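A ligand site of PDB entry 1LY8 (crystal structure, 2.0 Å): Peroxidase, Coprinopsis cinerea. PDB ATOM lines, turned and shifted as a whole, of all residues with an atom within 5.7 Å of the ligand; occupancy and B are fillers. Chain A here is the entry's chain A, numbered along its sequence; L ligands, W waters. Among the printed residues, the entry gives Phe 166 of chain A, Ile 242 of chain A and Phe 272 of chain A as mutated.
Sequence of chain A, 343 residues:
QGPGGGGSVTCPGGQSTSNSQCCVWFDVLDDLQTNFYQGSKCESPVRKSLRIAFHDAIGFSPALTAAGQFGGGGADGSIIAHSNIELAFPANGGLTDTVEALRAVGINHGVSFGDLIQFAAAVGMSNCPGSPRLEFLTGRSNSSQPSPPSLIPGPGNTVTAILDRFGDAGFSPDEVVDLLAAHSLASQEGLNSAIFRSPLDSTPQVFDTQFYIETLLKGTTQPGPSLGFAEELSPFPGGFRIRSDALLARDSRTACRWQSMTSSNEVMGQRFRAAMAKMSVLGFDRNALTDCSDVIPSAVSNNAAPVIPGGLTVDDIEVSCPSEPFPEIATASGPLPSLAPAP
A ring nitrogen (NE2) of His 183 is bound to an iron atom (FE1) of the ligand (2.2 Å).
An oxygen (O4) of the ligand lies within salt-bridge range of the guanidinium group (NE) of Arg 47, at 2.6 Å.
The backbone NH of Ser 187 lies within hydrogen-bond range of an oxygen (O4) of the ligand, 3.2 Å away.
OG of Ser 187 lies within hydrogen-bond range of O4 of the ligand (2.7 Å).
The backbone NH (N) of Gly 190 sits at hydrogen-bond distance from an oxygen (O1) of the ligand (2.7 Å).
An oxygen (O2) of the ligand sits at hydrogen-bond distance from the backbone NH (N) of Glu 189 (2.8 Å).
An oxygen (O1) of the ligand sits at hydrogen-bond distance from the backbone NH (N) of Leu 191 (3.3 Å).
A ring nitrogen (ND1) of His 183 is in hydrogen-bond range of the side-chain carboxylate (OD1) of Asp 245, at 2.7 Å.
NE of Arg 47 is in hydrogen-bond range of OG of Ser 187.
The side-chain amino group (NZ) of Lys 48 is in salt-bridge range of the side-chain carboxylate (OE1) of Glu 189 (2.8 Å).
The side-chain amide oxygen (OE1) of Gln 188 is in hydrogen-bond range of the backbone NH (N) of Leu 191 (2.9 Å).
The backbone carbonyl oxygen of Pro 155 lies within hydrogen-bond range of the backbone NH of Ser 244 (3.3 Å).
N of Leu 200 is in hydrogen-bond range of O of Ala 186, at 2.9 Å.
The guanidinium group (NH2) of Arg 51 is in hydrogen-bond range of the backbone carbonyl oxygen (O) of Gly 93, 2.7 Å away.
Merely in contact with the ligand: Lys 48 (3.6 Å), Leu 50 (3.6 Å), Arg 51 (3.8 Å), Phe 54 (3.5 Å), Pro 153 (3.8 Å), Gly 154 (3.4 Å), Pro 155 (3.4 Å), Ile 162 (3.9 Å), Phe 166 (3.4 Å), Leu 179 (3.8 Å), Leu 180 (3.5 Å), Ala 182 (3.6 Å), Leu 185 (3.6 Å), Ala 186 (3.4 Å), Gln 188 (3.6 Å), Ile 242 (3.9 Å), Ser 244 (3.4 Å), Phe 272 (3.8 Å), Met 276 (3.5 Å) and Met 279 (3.998 Å).
Hydrophobic or aromatic side chains within 4 Å of the ligand: Leu 50, Phe 54, Pro 155, Ile 162, Phe 166, Leu 179, Leu 180, Ala 182, His 183, Ala 186, Leu 191, Ile 242, Phe 272, Met 276 and Met 279.
Along chain A the residues within 4 Å of the ligand span positions 47 to 279.
Water W5 lies within hydrogen-bond range of O3 of the ligand, OE2 of Glu 189, OG of Ser 44 and NH2 of Arg 47.
Water W3 lies within hydrogen-bond range of O3 of the ligand (2.7 Å), NZ of Lys 48 (2.8 Å) and NH1 of Arg 51 (3.0 Å).
Water W4 lies within hydrogen-bond range of O2 of the ligand (2.9 Å), O of Gly 93 (3.1 Å) and NH1 of Arg 51 (3.2 Å).
Water W2 lies within hydrogen-bond range of the side-chain carboxylate of Asp 245 (2.6 Å) and the side-chain hydroxyl of Ser 244 (2.7 Å).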
ATOM      1  N   SER A  44      20.145  -8.129 -11.630  1.00  0.00           N
ATOM      2  CA  SER A  44      19.723  -7.341 -10.481  1.00  0.00           C
ATOM      3  C   SER A  44      18.307  -7.586  -9.971  1.00  0.00           C
ATOM      4  O   SER A  44      18.107  -7.811  -8.778  1.00  0.00           O
ATOM      5  CB  SER A  44      19.903  -5.844 -10.759  1.00  0.00           C
ATOM      6  OG  SER A  44      19.547  -5.088  -9.614  1.00  0.00           O
ATOM      7  N   VAL A  46      16.462 -10.121  -9.920  1.00  0.00           N
ATOM      8  CA  VAL A  46      16.346 -11.363  -9.153  1.00  0.00           C
ATOM      9  C   VAL A  46      16.872 -11.154  -7.745  1.00  0.00           C
ATOM     10  O   VAL A  46      16.248 -11.556  -6.763  1.00  0.00           O
ATOM     11  CB  VAL A  46      17.144 -12.516  -9.812  1.00  0.00           C
ATOM     12  CG1 VAL A  46      17.161 -13.719  -8.882  1.00  0.00           C
ATOM     13  CG2 VAL A  46      16.519 -12.899 -11.148  1.00  0.00           C
ATOM     14  N   ARG A  47      18.038 -10.508  -7.647  1.00  0.00           N
ATOM     15  CA  ARG A  47      18.645 -10.254  -6.361  1.00  0.00           C
ATOM     16  C   ARG A  47      17.781  -9.303  -5.528  1.00  0.00           C
ATOM     17  O   ARG A  47      17.571  -9.533  -4.342  1.00  0.00           O
ATOM     18  CB  ARG A  47      20.061  -9.682  -6.558  1.00  0.00           C
ATOM     19  CG  ARG A  47      20.957 -10.562  -7.444  1.00  0.00           C
ATOM     20  CD  ARG A  47      22.433 -10.144  -7.390  1.00  0.00           C
ATOM     21  NE  ARG A  47      22.668  -8.797  -7.898  1.00  0.00           N
ATOM     22  CZ  ARG A  47      22.863  -8.484  -9.174  1.00  0.00           C
ATOM     23  NH1 ARG A  47      22.860  -9.431 -10.102  1.00  0.00           N
ATOM     24  NH2 ARG A  47      23.042  -7.213  -9.530  1.00  0.00           N
ATOM     25  N   LYS A  48      17.256  -8.264  -6.160  1.00  0.00           N
ATOM     26  CA  LYS A  48      16.396  -7.315  -5.462  1.00  0.00           C
ATOM     27  C   LYS A  48      15.144  -8.014  -4.950  1.00  0.00           C
ATOM     28  O   LYS A  48      14.684  -7.767  -3.840  1.00  0.00           O
ATOM     29  CB  LYS A  48      15.996  -6.169  -6.396  1.00  0.00           C
ATOM     30  CG  LYS A  48      17.154  -5.273  -6.845  1.00  0.00           C
ATOM     31  CD  LYS A  48      17.707  -4.460  -5.692  1.00  0.00           C
ATOM     32  CE  LYS A  48      18.777  -3.481  -6.176  1.00  0.00           C
ATOM     33  NZ  LYS A  48      19.199  -2.537  -5.090  1.00  0.00           N
ATOM     34  N   LEU A  50      14.719 -11.264  -4.161  1.00  0.00           N
ATOM     35  CA  LEU A  50      15.063 -12.133  -3.032  1.00  0.00           C
ATOM     36  C   LEU A  50      15.218 -11.317  -1.753  1.00  0.00           C
ATOM     37  O   LEU A  50      14.747 -11.694  -0.684  1.00  0.00           O
ATOM     38  CB  LEU A  50      16.368 -12.867  -3.295  1.00  0.00           C
ATOM     39  CG  LEU A  50      16.285 -14.327  -3.748  1.00  0.00           C
ATOM     40  CD1 LEU A  50      17.665 -14.788  -4.189  1.00  0.00           C
ATOM     41  CD2 LEU A  50      15.752 -15.177  -2.609  1.00  0.00           C
ATOM     42  N   ARG A  51      15.897 -10.180  -1.879  1.00  0.00           N
ATOM     43  CA  ARG A  51      16.116  -9.304  -0.751  1.00  0.00           C
ATOM     44  C   ARG A  51      14.764  -8.833  -0.204  1.00  0.00           C
ATOM     45  O   ARG A  51      14.540  -8.810   1.002  1.00  0.00           O
ATOM     46  CB  ARG A  51      16.963  -8.109  -1.188  1.00  0.00           C
ATOM     47  CG  ARG A  51      17.409  -7.202  -0.050  1.00  0.00           C
ATOM     48  CD  ARG A  51      18.243  -6.047  -0.577  1.00  0.00           C
ATOM     49  NE  ARG A  51      18.333  -4.980   0.402  1.00  0.00           N
ATOM     50  CZ  ARG A  51      18.462  -3.693   0.094  1.00  0.00           C
ATOM     51  NH1 ARG A  51      18.536  -3.311  -1.181  1.00  0.00           N
ATOM     52  NH2 ARG A  51      18.520  -2.780   1.054  1.00  0.00           N
ATOM     53  N   PHE A  54      12.744 -11.407   1.837  1.00  0.00           N
ATOM     54  CA  PHE A  54      13.240 -11.482   3.205  1.00  0.00           C
ATOM     55  C   PHE A  54      12.722 -10.312   4.031  1.00  0.00           C
ATOM     56  O   PHE A  54      12.089 -10.494   5.071  1.00  0.00           O
ATOM     57  CB  PHE A  54      14.766 -11.490   3.201  1.00  0.00           C
ATOM     58  CG  PHE A  54      15.391 -11.370   4.573  1.00  0.00           C
ATOM     59  CD1 PHE A  54      16.525 -10.577   4.754  1.00  0.00           C
ATOM     60  CD2 PHE A  54      14.865 -12.045   5.666  1.00  0.00           C
ATOM     61  CE1 PHE A  54      17.123 -10.460   6.013  1.00  0.00           C
ATOM     62  CE2 PHE A  54      15.451 -11.940   6.926  1.00  0.00           C
ATOM     63  CZ  PHE A  54      16.585 -11.147   7.106  1.00  0.00           C
ATOM     64  N   HIS A  55      12.988  -9.089   3.567  1.00  0.00           N
ATOM     65  CA  HIS A  55      12.569  -7.889   4.301  1.00  0.00           C
ATOM     66  C   HIS A  55      11.069  -7.729   4.524  1.00  0.00           C
ATOM     67  O   HIS A  55      10.648  -6.985   5.420  1.00  0.00           O
ATOM     68  CB  HIS A  55      13.157  -6.647   3.636  1.00  0.00           C
ATOM     69  CG  HIS A  55      14.646  -6.543   3.738  1.00  0.00           C
ATOM     70  ND1 HIS A  55      15.349  -5.431   3.352  1.00  0.00           N
ATOM     71  CD2 HIS A  55      15.563  -7.436   4.185  1.00  0.00           C
ATOM     72  CE1 HIS A  55      16.647  -5.636   3.554  1.00  0.00           C
ATOM     73  NE2 HIS A  55      16.797  -6.848   4.054  1.00  0.00           N
ATOM     74  N   GLY A  93      16.945   0.313   1.793  1.00  0.00           N
ATOM     75  CA  GLY A  93      17.365   1.229   0.748  1.00  0.00           C
ATOM     76  C   GLY A  93      17.617   0.494  -0.556  1.00  0.00           C
ATOM     77  O   GLY A  93      17.924  -0.704  -0.542  1.00  0.00           O
ATOM     78  N   PRO A 153      17.430  -7.565  10.621  1.00  0.00           N
ATOM     79  CA  PRO A 153      18.822  -7.640  11.086  1.00  0.00           C
ATOM     80  C   PRO A 153      19.726  -6.758  10.222  1.00  0.00           C
ATOM     81  O   PRO A 153      19.583  -6.735   8.999  1.00  0.00           O
ATOM     82  CB  PRO A 153      19.152  -9.124  10.933  1.00  0.00           C
ATOM     83  CG  PRO A 153      17.834  -9.778  11.180  1.00  0.00           C
ATOM     84  CD  PRO A 153      16.903  -8.918  10.366  1.00  0.00           C
ATOM     85  N   GLY A 154      20.653  -6.045  10.864  1.00  0.00           N
ATOM     86  CA  GLY A 154      21.562  -5.169  10.157  1.00  0.00           C
ATOM     87  C   GLY A 154      22.971  -5.726   9.999  1.00  0.00           C
ATOM     88  O   GLY A 154      23.428  -6.506  10.834  1.00  0.00           O
ATOM     89  N   PRO A 155      23.699  -5.323   8.940  1.00  0.00           N
ATOM     90  CA  PRO A 155      25.060  -5.805   8.706  1.00  0.00           C
ATOM     91  C   PRO A 155      26.058  -5.477   9.812  1.00  0.00           C
ATOM     92  O   PRO A 155      27.089  -6.134   9.936  1.00  0.00           O
ATOM     93  CB  PRO A 155      25.430  -5.142   7.377  1.00  0.00           C
ATOM     94  CG  PRO A 155      24.668  -3.857   7.434  1.00  0.00           C
ATOM     95  CD  PRO A 155      23.324  -4.291   7.950  1.00  0.00           C
ATOM     96  N   GLY A 156      25.739  -4.466  10.623  1.00  0.00           N
ATOM     97  CA  GLY A 156      26.643  -4.097  11.696  1.00  0.00           C
ATOM     98  C   GLY A 156      26.297  -4.736  13.024  1.00  0.00           C
ATOM     99  O   GLY A 156      26.982  -4.496  14.016  1.00  0.00           O
ATOM    100  N   ILE A 162      21.820 -10.827  15.871  1.00  0.00           N
ATOM    101  CA  ILE A 162      21.251 -11.481  14.695  1.00  0.00           C
ATOM    102  C   ILE A 162      20.532 -12.777  15.077  1.00  0.00           C
ATOM    103  O   ILE A 162      19.405 -13.026  14.637  1.00  0.00           O
ATOM    104  CB  ILE A 162      22.340 -11.776  13.643  1.00  0.00           C
ATOM    105  CG1 ILE A 162      22.895 -10.466  13.087  1.00  0.00           C
ATOM    106  CG2 ILE A 162      21.780 -12.637  12.514  1.00  0.00           C
ATOM    107  CD1 ILE A 162      24.110 -10.628  12.200  1.00  0.00           C
ATOM    108  N   PHE A 166      16.386 -13.468  14.638  1.00  0.00           N
ATOM    109  CA  PHE A 166      15.907 -14.654  13.920  1.00  0.00           C
ATOM    110  C   PHE A 166      15.239 -15.623  14.893  1.00  0.00           C
ATOM    111  O   PHE A 166      14.218 -16.225  14.576  1.00  0.00           O
ATOM    112  CB  PHE A 166      17.060 -15.341  13.191  1.00  0.00           C
ATOM    113  CG  PHE A 166      17.369 -14.748  11.844  1.00  0.00           C
ATOM    114  CD1 PHE A 166      16.544 -15.002  10.751  1.00  0.00           C
ATOM    115  CD2 PHE A 166      18.468 -13.920  11.675  1.00  0.00           C
ATOM    116  CE1 PHE A 166      16.815 -14.440   9.505  1.00  0.00           C
ATOM    117  CE2 PHE A 166      18.751 -13.346  10.427  1.00  0.00           C
ATOM    118  CZ  PHE A 166      17.914 -13.612   9.335  1.00  0.00           C
ATOM    119  N   VAL A 176      19.584 -19.839  10.174  1.00  0.00           N
ATOM    120  CA  VAL A 176      20.046 -18.513   9.764  1.00  0.00           C
ATOM    121  C   VAL A 176      21.157 -18.717   8.742  1.00  0.00           C
ATOM    122  O   VAL A 176      21.193 -18.066   7.698  1.00  0.00           O
ATOM    123  CB  VAL A 176      20.588 -17.696  10.958  1.00  0.00           C
ATOM    124  CG1 VAL A 176      21.067 -16.334  10.490  1.00  0.00           C
ATOM    125  CG2 VAL A 176      19.496 -17.550  12.026  1.00  0.00           C
ATOM    126  N   LEU A 179      19.679 -19.831   5.527  1.00  0.00           N
ATOM    127  CA  LEU A 179      19.005 -18.705   4.894  1.00  0.00           C
ATOM    128  C   LEU A 179      19.980 -17.806   4.137  1.00  0.00           C
ATOM    129  O   LEU A 179      19.646 -17.265   3.085  1.00  0.00           O
ATOM    130  CB  LEU A 179      18.255 -17.895   5.957  1.00  0.00           C
ATOM    131  CG  LEU A 179      16.731 -17.748   5.896  1.00  0.00           C
ATOM    132  CD1 LEU A 179      16.102 -18.820   5.027  1.00  0.00           C
ATOM    133  CD2 LEU A 179      16.187 -17.800   7.320  1.00  0.00           C
ATOM    134  N   LEU A 180      21.190 -17.657   4.677  1.00  0.00           N
ATOM    135  CA  LEU A 180      22.193 -16.811   4.065  1.00  0.00           C
ATOM    136  C   LEU A 180      22.739 -17.341   2.733  1.00  0.00           C
ATOM    137  O   LEU A 180      23.536 -16.668   2.071  1.00  0.00           O
ATOM    138  CB  LEU A 180      23.333 -16.568   5.051  1.00  0.00           C
ATOM    139  CG  LEU A 180      23.022 -15.468   6.063  1.00  0.00           C
ATOM    140  CD1 LEU A 180      24.121 -15.360   7.099  1.00  0.00           C
ATOM    141  CD2 LEU A 180      22.874 -14.164   5.309  1.00  0.00           C
ATOM    142  N   ALA A 182      21.380 -17.316   0.218  1.00  0.00           N
ATOM    143  CA  ALA A 182      20.904 -16.356  -0.785  1.00  0.00           C
ATOM    144  C   ALA A 182      22.010 -15.392  -1.182  1.00  0.00           C
ATOM    145  O   ALA A 182      21.950 -14.777  -2.247  1.00  0.00           O
ATOM    146  CB  ALA A 182      19.707 -15.595  -0.252  1.00  0.00           C
ATOM    147  N   HIS A 183      23.019 -15.245  -0.341  1.00  0.00           N
ATOM    148  CA  HIS A 183      24.113 -14.339  -0.657  1.00  0.00           C
ATOM    149  C   HIS A 183      25.040 -14.911  -1.724  1.00  0.00           C
ATOM    150  O   HIS A 183      26.033 -14.294  -2.095  1.00  0.00           O
ATOM    151  CB  HIS A 183      24.899 -13.977   0.605  1.00  0.00           C
ATOM    152  CG  HIS A 183      24.273 -12.864   1.390  1.00  0.00           C
ATOM    153  ND1 HIS A 183      24.898 -12.205   2.419  1.00  0.00           N
ATOM    154  CD2 HIS A 183      23.045 -12.299   1.275  1.00  0.00           C
ATOM    155  CE1 HIS A 183      24.052 -11.270   2.892  1.00  0.00           C
ATOM    156  NE2 HIS A 183      22.915 -11.288   2.225  1.00  0.00           N
ATOM    157  N   LEU A 185      24.029 -15.257  -4.550  1.00  0.00           N
ATOM    158  CA  LEU A 185      23.502 -14.535  -5.716  1.00  0.00           C
ATOM    159  C   LEU A 185      23.317 -13.105  -5.239  1.00  0.00           C
ATOM    160  O   LEU A 185      22.221 -12.530  -5.338  1.00  0.00           O
ATOM    161  CB  LEU A 185      22.136 -15.098  -6.135  1.00  0.00           C
ATOM    162  CG  LEU A 185      22.004 -16.593  -6.452  1.00  0.00           C
ATOM    163  CD1 LEU A 185      20.524 -16.917  -6.611  1.00  0.00           C
ATOM    164  CD2 LEU A 185      22.779 -16.932  -7.713  1.00  0.00           C
ATOM    165  N   ALA A 186      24.381 -12.512  -4.722  1.00  0.00           N
ATOM    166  CA  ALA A 186      24.292 -11.164  -4.167  1.00  0.00           C
ATOM    167  C   ALA A 186      25.442 -10.222  -4.469  1.00  0.00           C
ATOM    168  O   ALA A 186      26.555 -10.632  -4.826  1.00  0.00           O
ATOM    169  CB  ALA A 186      24.112 -11.266  -2.662  1.00  0.00           C
ATOM    170  N   SER A 187      25.141  -8.949  -4.282  1.00  0.00           N
ATOM    171  CA  SER A 187      26.086  -7.863  -4.477  1.00  0.00           C
ATOM    172  C   SER A 187      25.579  -6.746  -3.562  1.00  0.00           C
ATOM    173  O   SER A 187      24.552  -6.918  -2.871  1.00  0.00           O
ATOM    174  CB  SER A 187      26.067  -7.391  -5.930  1.00  0.00           C
ATOM    175  OG  SER A 187      24.861  -6.718  -6.228  1.00  0.00           O
ATOM    176  N   GLN A 188      26.261  -5.623  -3.538  1.00  0.00           N
ATOM    177  CA  GLN A 188      25.815  -4.513  -2.714  1.00  0.00           C
ATOM    178  C   GLN A 188      25.855  -3.249  -3.554  1.00  0.00           C
ATOM    179  O   GLN A 188      26.690  -3.117  -4.445  1.00  0.00           O
ATOM    180  CB  GLN A 188      26.712  -4.363  -1.472  1.00  0.00           C
ATOM    181  CG  GLN A 188      28.152  -3.914  -1.746  1.00  0.00           C
ATOM    182  CD  GLN A 188      28.269  -2.450  -2.129  1.00  0.00           C
ATOM    183  OE1 GLN A 188      27.541  -1.601  -1.606  1.00  0.00           O
ATOM    184  NE2 GLN A 188      29.192  -2.131  -3.029  1.00  0.00           N
ATOM    185  N   GLU A 189      24.942  -2.330  -3.280  1.00  0.00           N
ATOM    186  CA  GLU A 189      24.888  -1.067  -4.001  1.00  0.00           C
ATOM    187  C   GLU A 189      24.879   0.086  -3.015  1.00  0.00           C
ATOM    188  O   GLU A 189      25.344   1.181  -3.319  1.00  0.00           O
ATOM    189  CB  GLU A 189      23.633  -0.970  -4.868  1.00  0.00           C
ATOM    190  CG  GLU A 189      23.312  -2.201  -5.694  1.00  0.00           C
ATOM    191  CD  GLU A 189      22.140  -1.972  -6.645  1.00  0.00           C
ATOM    192  OE1 GLU A 189      21.262  -1.140  -6.309  1.00  0.00           O
ATOM    193  OE2 GLU A 189      22.083  -2.625  -7.698  1.00  0.00           O
ATOM    194  N   GLY A 190      24.352  -0.167  -1.820  1.00  0.00           N
ATOM    195  CA  GLY A 190      24.245   0.873  -0.815  1.00  0.00           C
ATOM    196  C   GLY A 190      25.286   0.951   0.293  1.00  0.00           C
ATOM    197  O   GLY A 190      25.331   1.938   1.021  1.00  0.00           O
ATOM    198  N   LEU A 191      26.109  -0.081   0.442  1.00  0.00           N
ATOM    199  CA  LEU A 191      27.133  -0.068   1.489  1.00  0.00           C
ATOM    200  C   LEU A 191      28.348   0.751   1.089  1.00  0.00           C
ATOM    201  O   LEU A 191      28.945   1.453   1.909  1.00  0.00           O
ATOM    202  CB  LEU A 191      27.569  -1.497   1.817  1.00  0.00           C
ATOM    203  CG  LEU A 191      26.494  -2.418   2.418  1.00  0.00           C
ATOM    204  CD1 LEU A 191      27.102  -3.782   2.710  1.00  0.00           C
ATOM    205  CD2 LEU A 191      25.943  -1.798   3.680  1.00  0.00           C
ATOM    206  N   LEU A 200      29.167 -10.594  -3.678  1.00  0.00           N
ATOM    207  CA  LEU A 200      29.493 -11.214  -2.401  1.00  0.00           C
ATOM    208  C   LEU A 200      30.301 -12.486  -2.600  1.00  0.00           C
ATOM    209  O   LEU A 200      31.054 -12.892  -1.710  1.00  0.00           O
ATOM    210  CB  LEU A 200      28.231 -11.516  -1.594  1.00  0.00           C
ATOM    211  CG  LEU A 200      27.616 -10.334  -0.827  1.00  0.00           C
ATOM    212  CD1 LEU A 200      27.166  -9.262  -1.793  1.00  0.00           C
ATOM    213  CD2 LEU A 200      26.449 -10.814   0.000  1.00  0.00           C
ATOM    214  N   ILE A 242      30.592  -8.483   3.692  1.00  0.00           N
ATOM    215  CA  ILE A 242      29.775  -7.858   4.729  1.00  0.00           C
ATOM    216  C   ILE A 242      30.245  -8.381   6.088  1.00  0.00           C
ATOM    217  O   ILE A 242      30.435  -9.581   6.270  1.00  0.00           O
ATOM    218  CB  ILE A 242      28.282  -8.210   4.543  1.00  0.00           C
ATOM    219  CG1 ILE A 242      27.812  -7.767   3.154  1.00  0.00           C
ATOM    220  CG2 ILE A 242      27.450  -7.544   5.613  1.00  0.00           C
ATOM    221  CD1 ILE A 242      26.433  -8.269   2.774  1.00  0.00           C
ATOM    222  N   SER A 244      28.717  -8.839   8.982  1.00  0.00           N
ATOM    223  CA  SER A 244      27.862  -9.850   9.593  1.00  0.00           C
ATOM    224  C   SER A 244      28.096 -11.244   9.008  1.00  0.00           C
ATOM    225  O   SER A 244      28.039 -12.239   9.732  1.00  0.00           O
ATOM    226  CB  SER A 244      26.377  -9.457   9.433  1.00  0.00           C
ATOM    227  OG  SER A 244      26.017  -9.287   8.077  1.00  0.00           O
ATOM    228  N   ASP A 245      28.367 -11.308   7.706  1.00  0.00           N
ATOM    229  CA  ASP A 245      28.641 -12.590   7.052  1.00  0.00           C
ATOM    230  C   ASP A 245      29.970 -13.140   7.558  1.00  0.00           C
ATOM    231  O   ASP A 245      30.078 -14.327   7.872  1.00  0.00           O
ATOM    232  CB  ASP A 245      28.721 -12.409   5.533  1.00  0.00           C
ATOM    233  CG  ASP A 245      27.351 -12.297   4.890  1.00  0.00           C
ATOM    234  OD1 ASP A 245      27.294 -11.963   3.685  1.00  0.00           O
ATOM    235  OD2 ASP A 245      26.343 -12.550   5.579  1.00  0.00           O
ATOM    236  N   LEU A 248      29.478 -14.376  11.221  1.00  0.00           N
ATOM    237  CA  LEU A 248      28.680 -15.584  11.292  1.00  0.00           C
ATOM    238  C   LEU A 248      29.472 -16.803  10.842  1.00  0.00           C
ATOM    239  O   LEU A 248      29.314 -17.894  11.400  1.00  0.00           O
ATOM    240  CB  LEU A 248      27.423 -15.430  10.435  1.00  0.00           C
ATOM    241  CG  LEU A 248      26.417 -14.403  10.977  1.00  0.00           C
ATOM    242  CD1 LEU A 248      25.337 -14.114   9.932  1.00  0.00           C
ATOM    243  CD2 LEU A 248      25.813 -14.948  12.266  1.00  0.00           C
ATOM    244  N   PHE A 272      18.251 -24.523   2.110  1.00  0.00           N
ATOM    245  CA  PHE A 272      17.728 -23.202   1.793  1.00  0.00           C
ATOM    246  C   PHE A 272      16.241 -23.269   1.470  1.00  0.00           C
ATOM    247  O   PHE A 272      15.468 -22.399   1.884  1.00  0.00           O
ATOM    248  CB  PHE A 272      18.481 -22.587   0.617  1.00  0.00           C
ATOM    249  CG  PHE A 272      17.986 -21.231   0.228  1.00  0.00           C
ATOM    250  CD1 PHE A 272      17.153 -21.061  -0.869  1.00  0.00           C
ATOM    251  CD2 PHE A 272      18.323 -20.107   0.989  1.00  0.00           C
ATOM    252  CE1 PHE A 272      16.652 -19.802  -1.209  1.00  0.00           C
ATOM    253  CE2 PHE A 272      17.832 -18.849   0.663  1.00  0.00           C
ATOM    254  CZ  PHE A 272      16.996 -18.700  -0.439  1.00  0.00           C
ATOM    255  N   MET A 276      13.496 -21.326   3.573  1.00  0.00           N
ATOM    256  CA  MET A 276      12.690 -20.360   2.819  1.00  0.00           C
ATOM    257  C   MET A 276      11.206 -20.669   2.900  1.00  0.00           C
ATOM    258  O   MET A 276      10.369 -19.763   2.892  1.00  0.00           O
ATOM    259  CB  MET A 276      13.122 -20.322   1.352  1.00  0.00           C
ATOM    260  CG  MET A 276      14.271 -19.385   1.085  1.00  0.00           C
ATOM    261  SD  MET A 276      13.856 -17.674   1.491  1.00  0.00           S
ATOM    262  CE  MET A 276      13.188 -17.096  -0.066  1.00  0.00           C
ATOM    263  N   MET A 279      10.027 -19.147   6.023  1.00  0.00           N
ATOM    264  CA  MET A 279      10.052 -17.693   5.965  1.00  0.00           C
ATOM    265  C   MET A 279       8.894 -17.143   5.136  1.00  0.00           C
ATOM    266  O   MET A 279       8.248 -16.172   5.526  1.00  0.00           O
ATOM    267  CB  MET A 279      11.374 -17.217   5.360  1.00  0.00           C
ATOM    268  CG  MET A 279      11.451 -15.713   5.180  1.00  0.00           C
ATOM    269  SD  MET A 279      13.023 -15.208   4.494  1.00  0.00           S
ATOM    270  CE  MET A 279      14.065 -15.332   5.946  1.00  0.00           C
HETATM  271  C1  LIG L   1      22.092  -8.054   0.123  1.00  0.00           C
HETATM  272  C2  LIG L   1      22.465  -7.903   4.770  1.00  0.00           C
HETATM  273  C3  LIG L   1      20.104 -11.968   5.001  1.00  0.00           C
HETATM  274  C4  LIG L   1      19.183 -11.795   0.325  1.00  0.00           C
HETATM  275  C5  LIG L   1      22.401  -7.563   1.383  1.00  0.00           C
HETATM  276  C6  LIG L   1      23.008  -6.275   1.700  1.00  0.00           C
HETATM  277  C7  LIG L   1      23.087  -6.211   3.165  1.00  0.00           C
HETATM  278  C8  LIG L   1      22.552  -7.419   3.559  1.00  0.00           C
HETATM  279  C9  LIG L   1      23.761  -4.974   4.025  1.00  0.00           C
HETATM  280  C10 LIG L   1      23.497  -5.162   0.651  1.00  0.00           C
HETATM  281  C11 LIG L   1      22.246  -4.257   0.296  1.00  0.00           C
HETATM  282  C12 LIG L   1      22.945  -3.160  -0.734  1.00  0.00           C
HETATM  283  O1  LIG L   1      23.716  -2.303  -0.245  1.00  0.00           O
HETATM  284  O2  LIG L   1      22.549  -3.144  -2.004  1.00  0.00           O
HETATM  285  C13 LIG L   1      21.948  -9.088   5.362  1.00  0.00           C
HETATM  286  C14 LIG L   1      22.027  -9.379   6.741  1.00  0.00           C
HETATM  287  C15 LIG L   1      21.361 -10.713   6.829  1.00  0.00           C
HETATM  288  C16 LIG L   1      20.870 -10.948   5.444  1.00  0.00           C
HETATM  289  C17 LIG L   1      22.766  -8.453   7.983  1.00  0.00           C
HETATM  290  C18 LIG L   1      21.447 -11.312   8.113  1.00  0.00           C
HETATM  291  C19 LIG L   1      21.402 -12.255   8.672  1.00  0.00           C
HETATM  292  C20 LIG L   1      19.510 -12.328   3.771  1.00  0.00           C
HETATM  293  C21 LIG L   1      18.339 -13.428   3.622  1.00  0.00           C
HETATM  294  C22 LIG L   1      18.013 -13.308   2.227  1.00  0.00           C
HETATM  295  C23 LIG L   1      19.014 -12.194   1.677  1.00  0.00           C
HETATM  296  C24 LIG L   1      17.754 -14.275   4.823  1.00  0.00           C
HETATM  297  C25 LIG L   1      16.968 -13.963   1.430  1.00  0.00           C
HETATM  298  C26 LIG L   1      16.496 -15.366   1.448  1.00  0.00           C
HETATM  299  C27 LIG L   1      20.000 -10.851  -0.325  1.00  0.00           C
HETATM  300  C28 LIG L   1      20.199 -10.677  -1.763  1.00  0.00           C
HETATM  301  C29 LIG L   1      21.109  -9.463  -1.824  1.00  0.00           C
HETATM  302  C30 LIG L   1      21.351  -9.125  -0.401  1.00  0.00           C
HETATM  303  C31 LIG L   1      19.675 -11.576  -2.973  1.00  0.00           C
HETATM  304  C32 LIG L   1      21.654  -8.881  -2.982  1.00  0.00           C
HETATM  305  C33 LIG L   1      21.025  -7.561  -3.477  1.00  0.00           C
HETATM  306  C34 LIG L   1      21.589  -7.083  -4.791  1.00  0.00           C
HETATM  307  O3  LIG L   1      21.005  -6.194  -5.189  1.00  0.00           O
HETATM  308  O4  LIG L   1      22.444  -7.732  -5.507  1.00  0.00           O
HETATM  309  N1  LIG L   1      22.101  -8.227   2.387  1.00  0.00           N
HETATM  310  N2  LIG L   1      21.302 -10.043   4.605  1.00  0.00           N
HETATM  311  N3  LIG L   1      19.845 -11.655   2.646  1.00  0.00           N
HETATM  312  N4  LIG L   1      20.781  -9.937   0.444  1.00  0.00           N
HETATM  313 FE1  LIG L   1      21.136 -10.063   2.563  1.00  0.00          FE
HETATM  314  O   HOH W   1      19.895  -5.457   2.701  1.00  0.00           O
HETATM  315  O   HOH W   2      24.760 -11.561   7.323  1.00  0.00           O
HETATM  316  O   HOH W   3      20.429  -4.325  -3.315  1.00  0.00           O
HETATM  317  O   HOH W   4      20.653  -1.006  -2.035  1.00  0.00           O
HETATM  318  O   HOH W   5      21.734  -5.296  -7.609  1.00  0.00           O
HETATM  319  O   HOH W   6      19.220  -7.375   4.971  1.00  0.00           O
HETATM  320  O   HOH W   7      22.909  -1.019   2.056  1.00  0.00           O
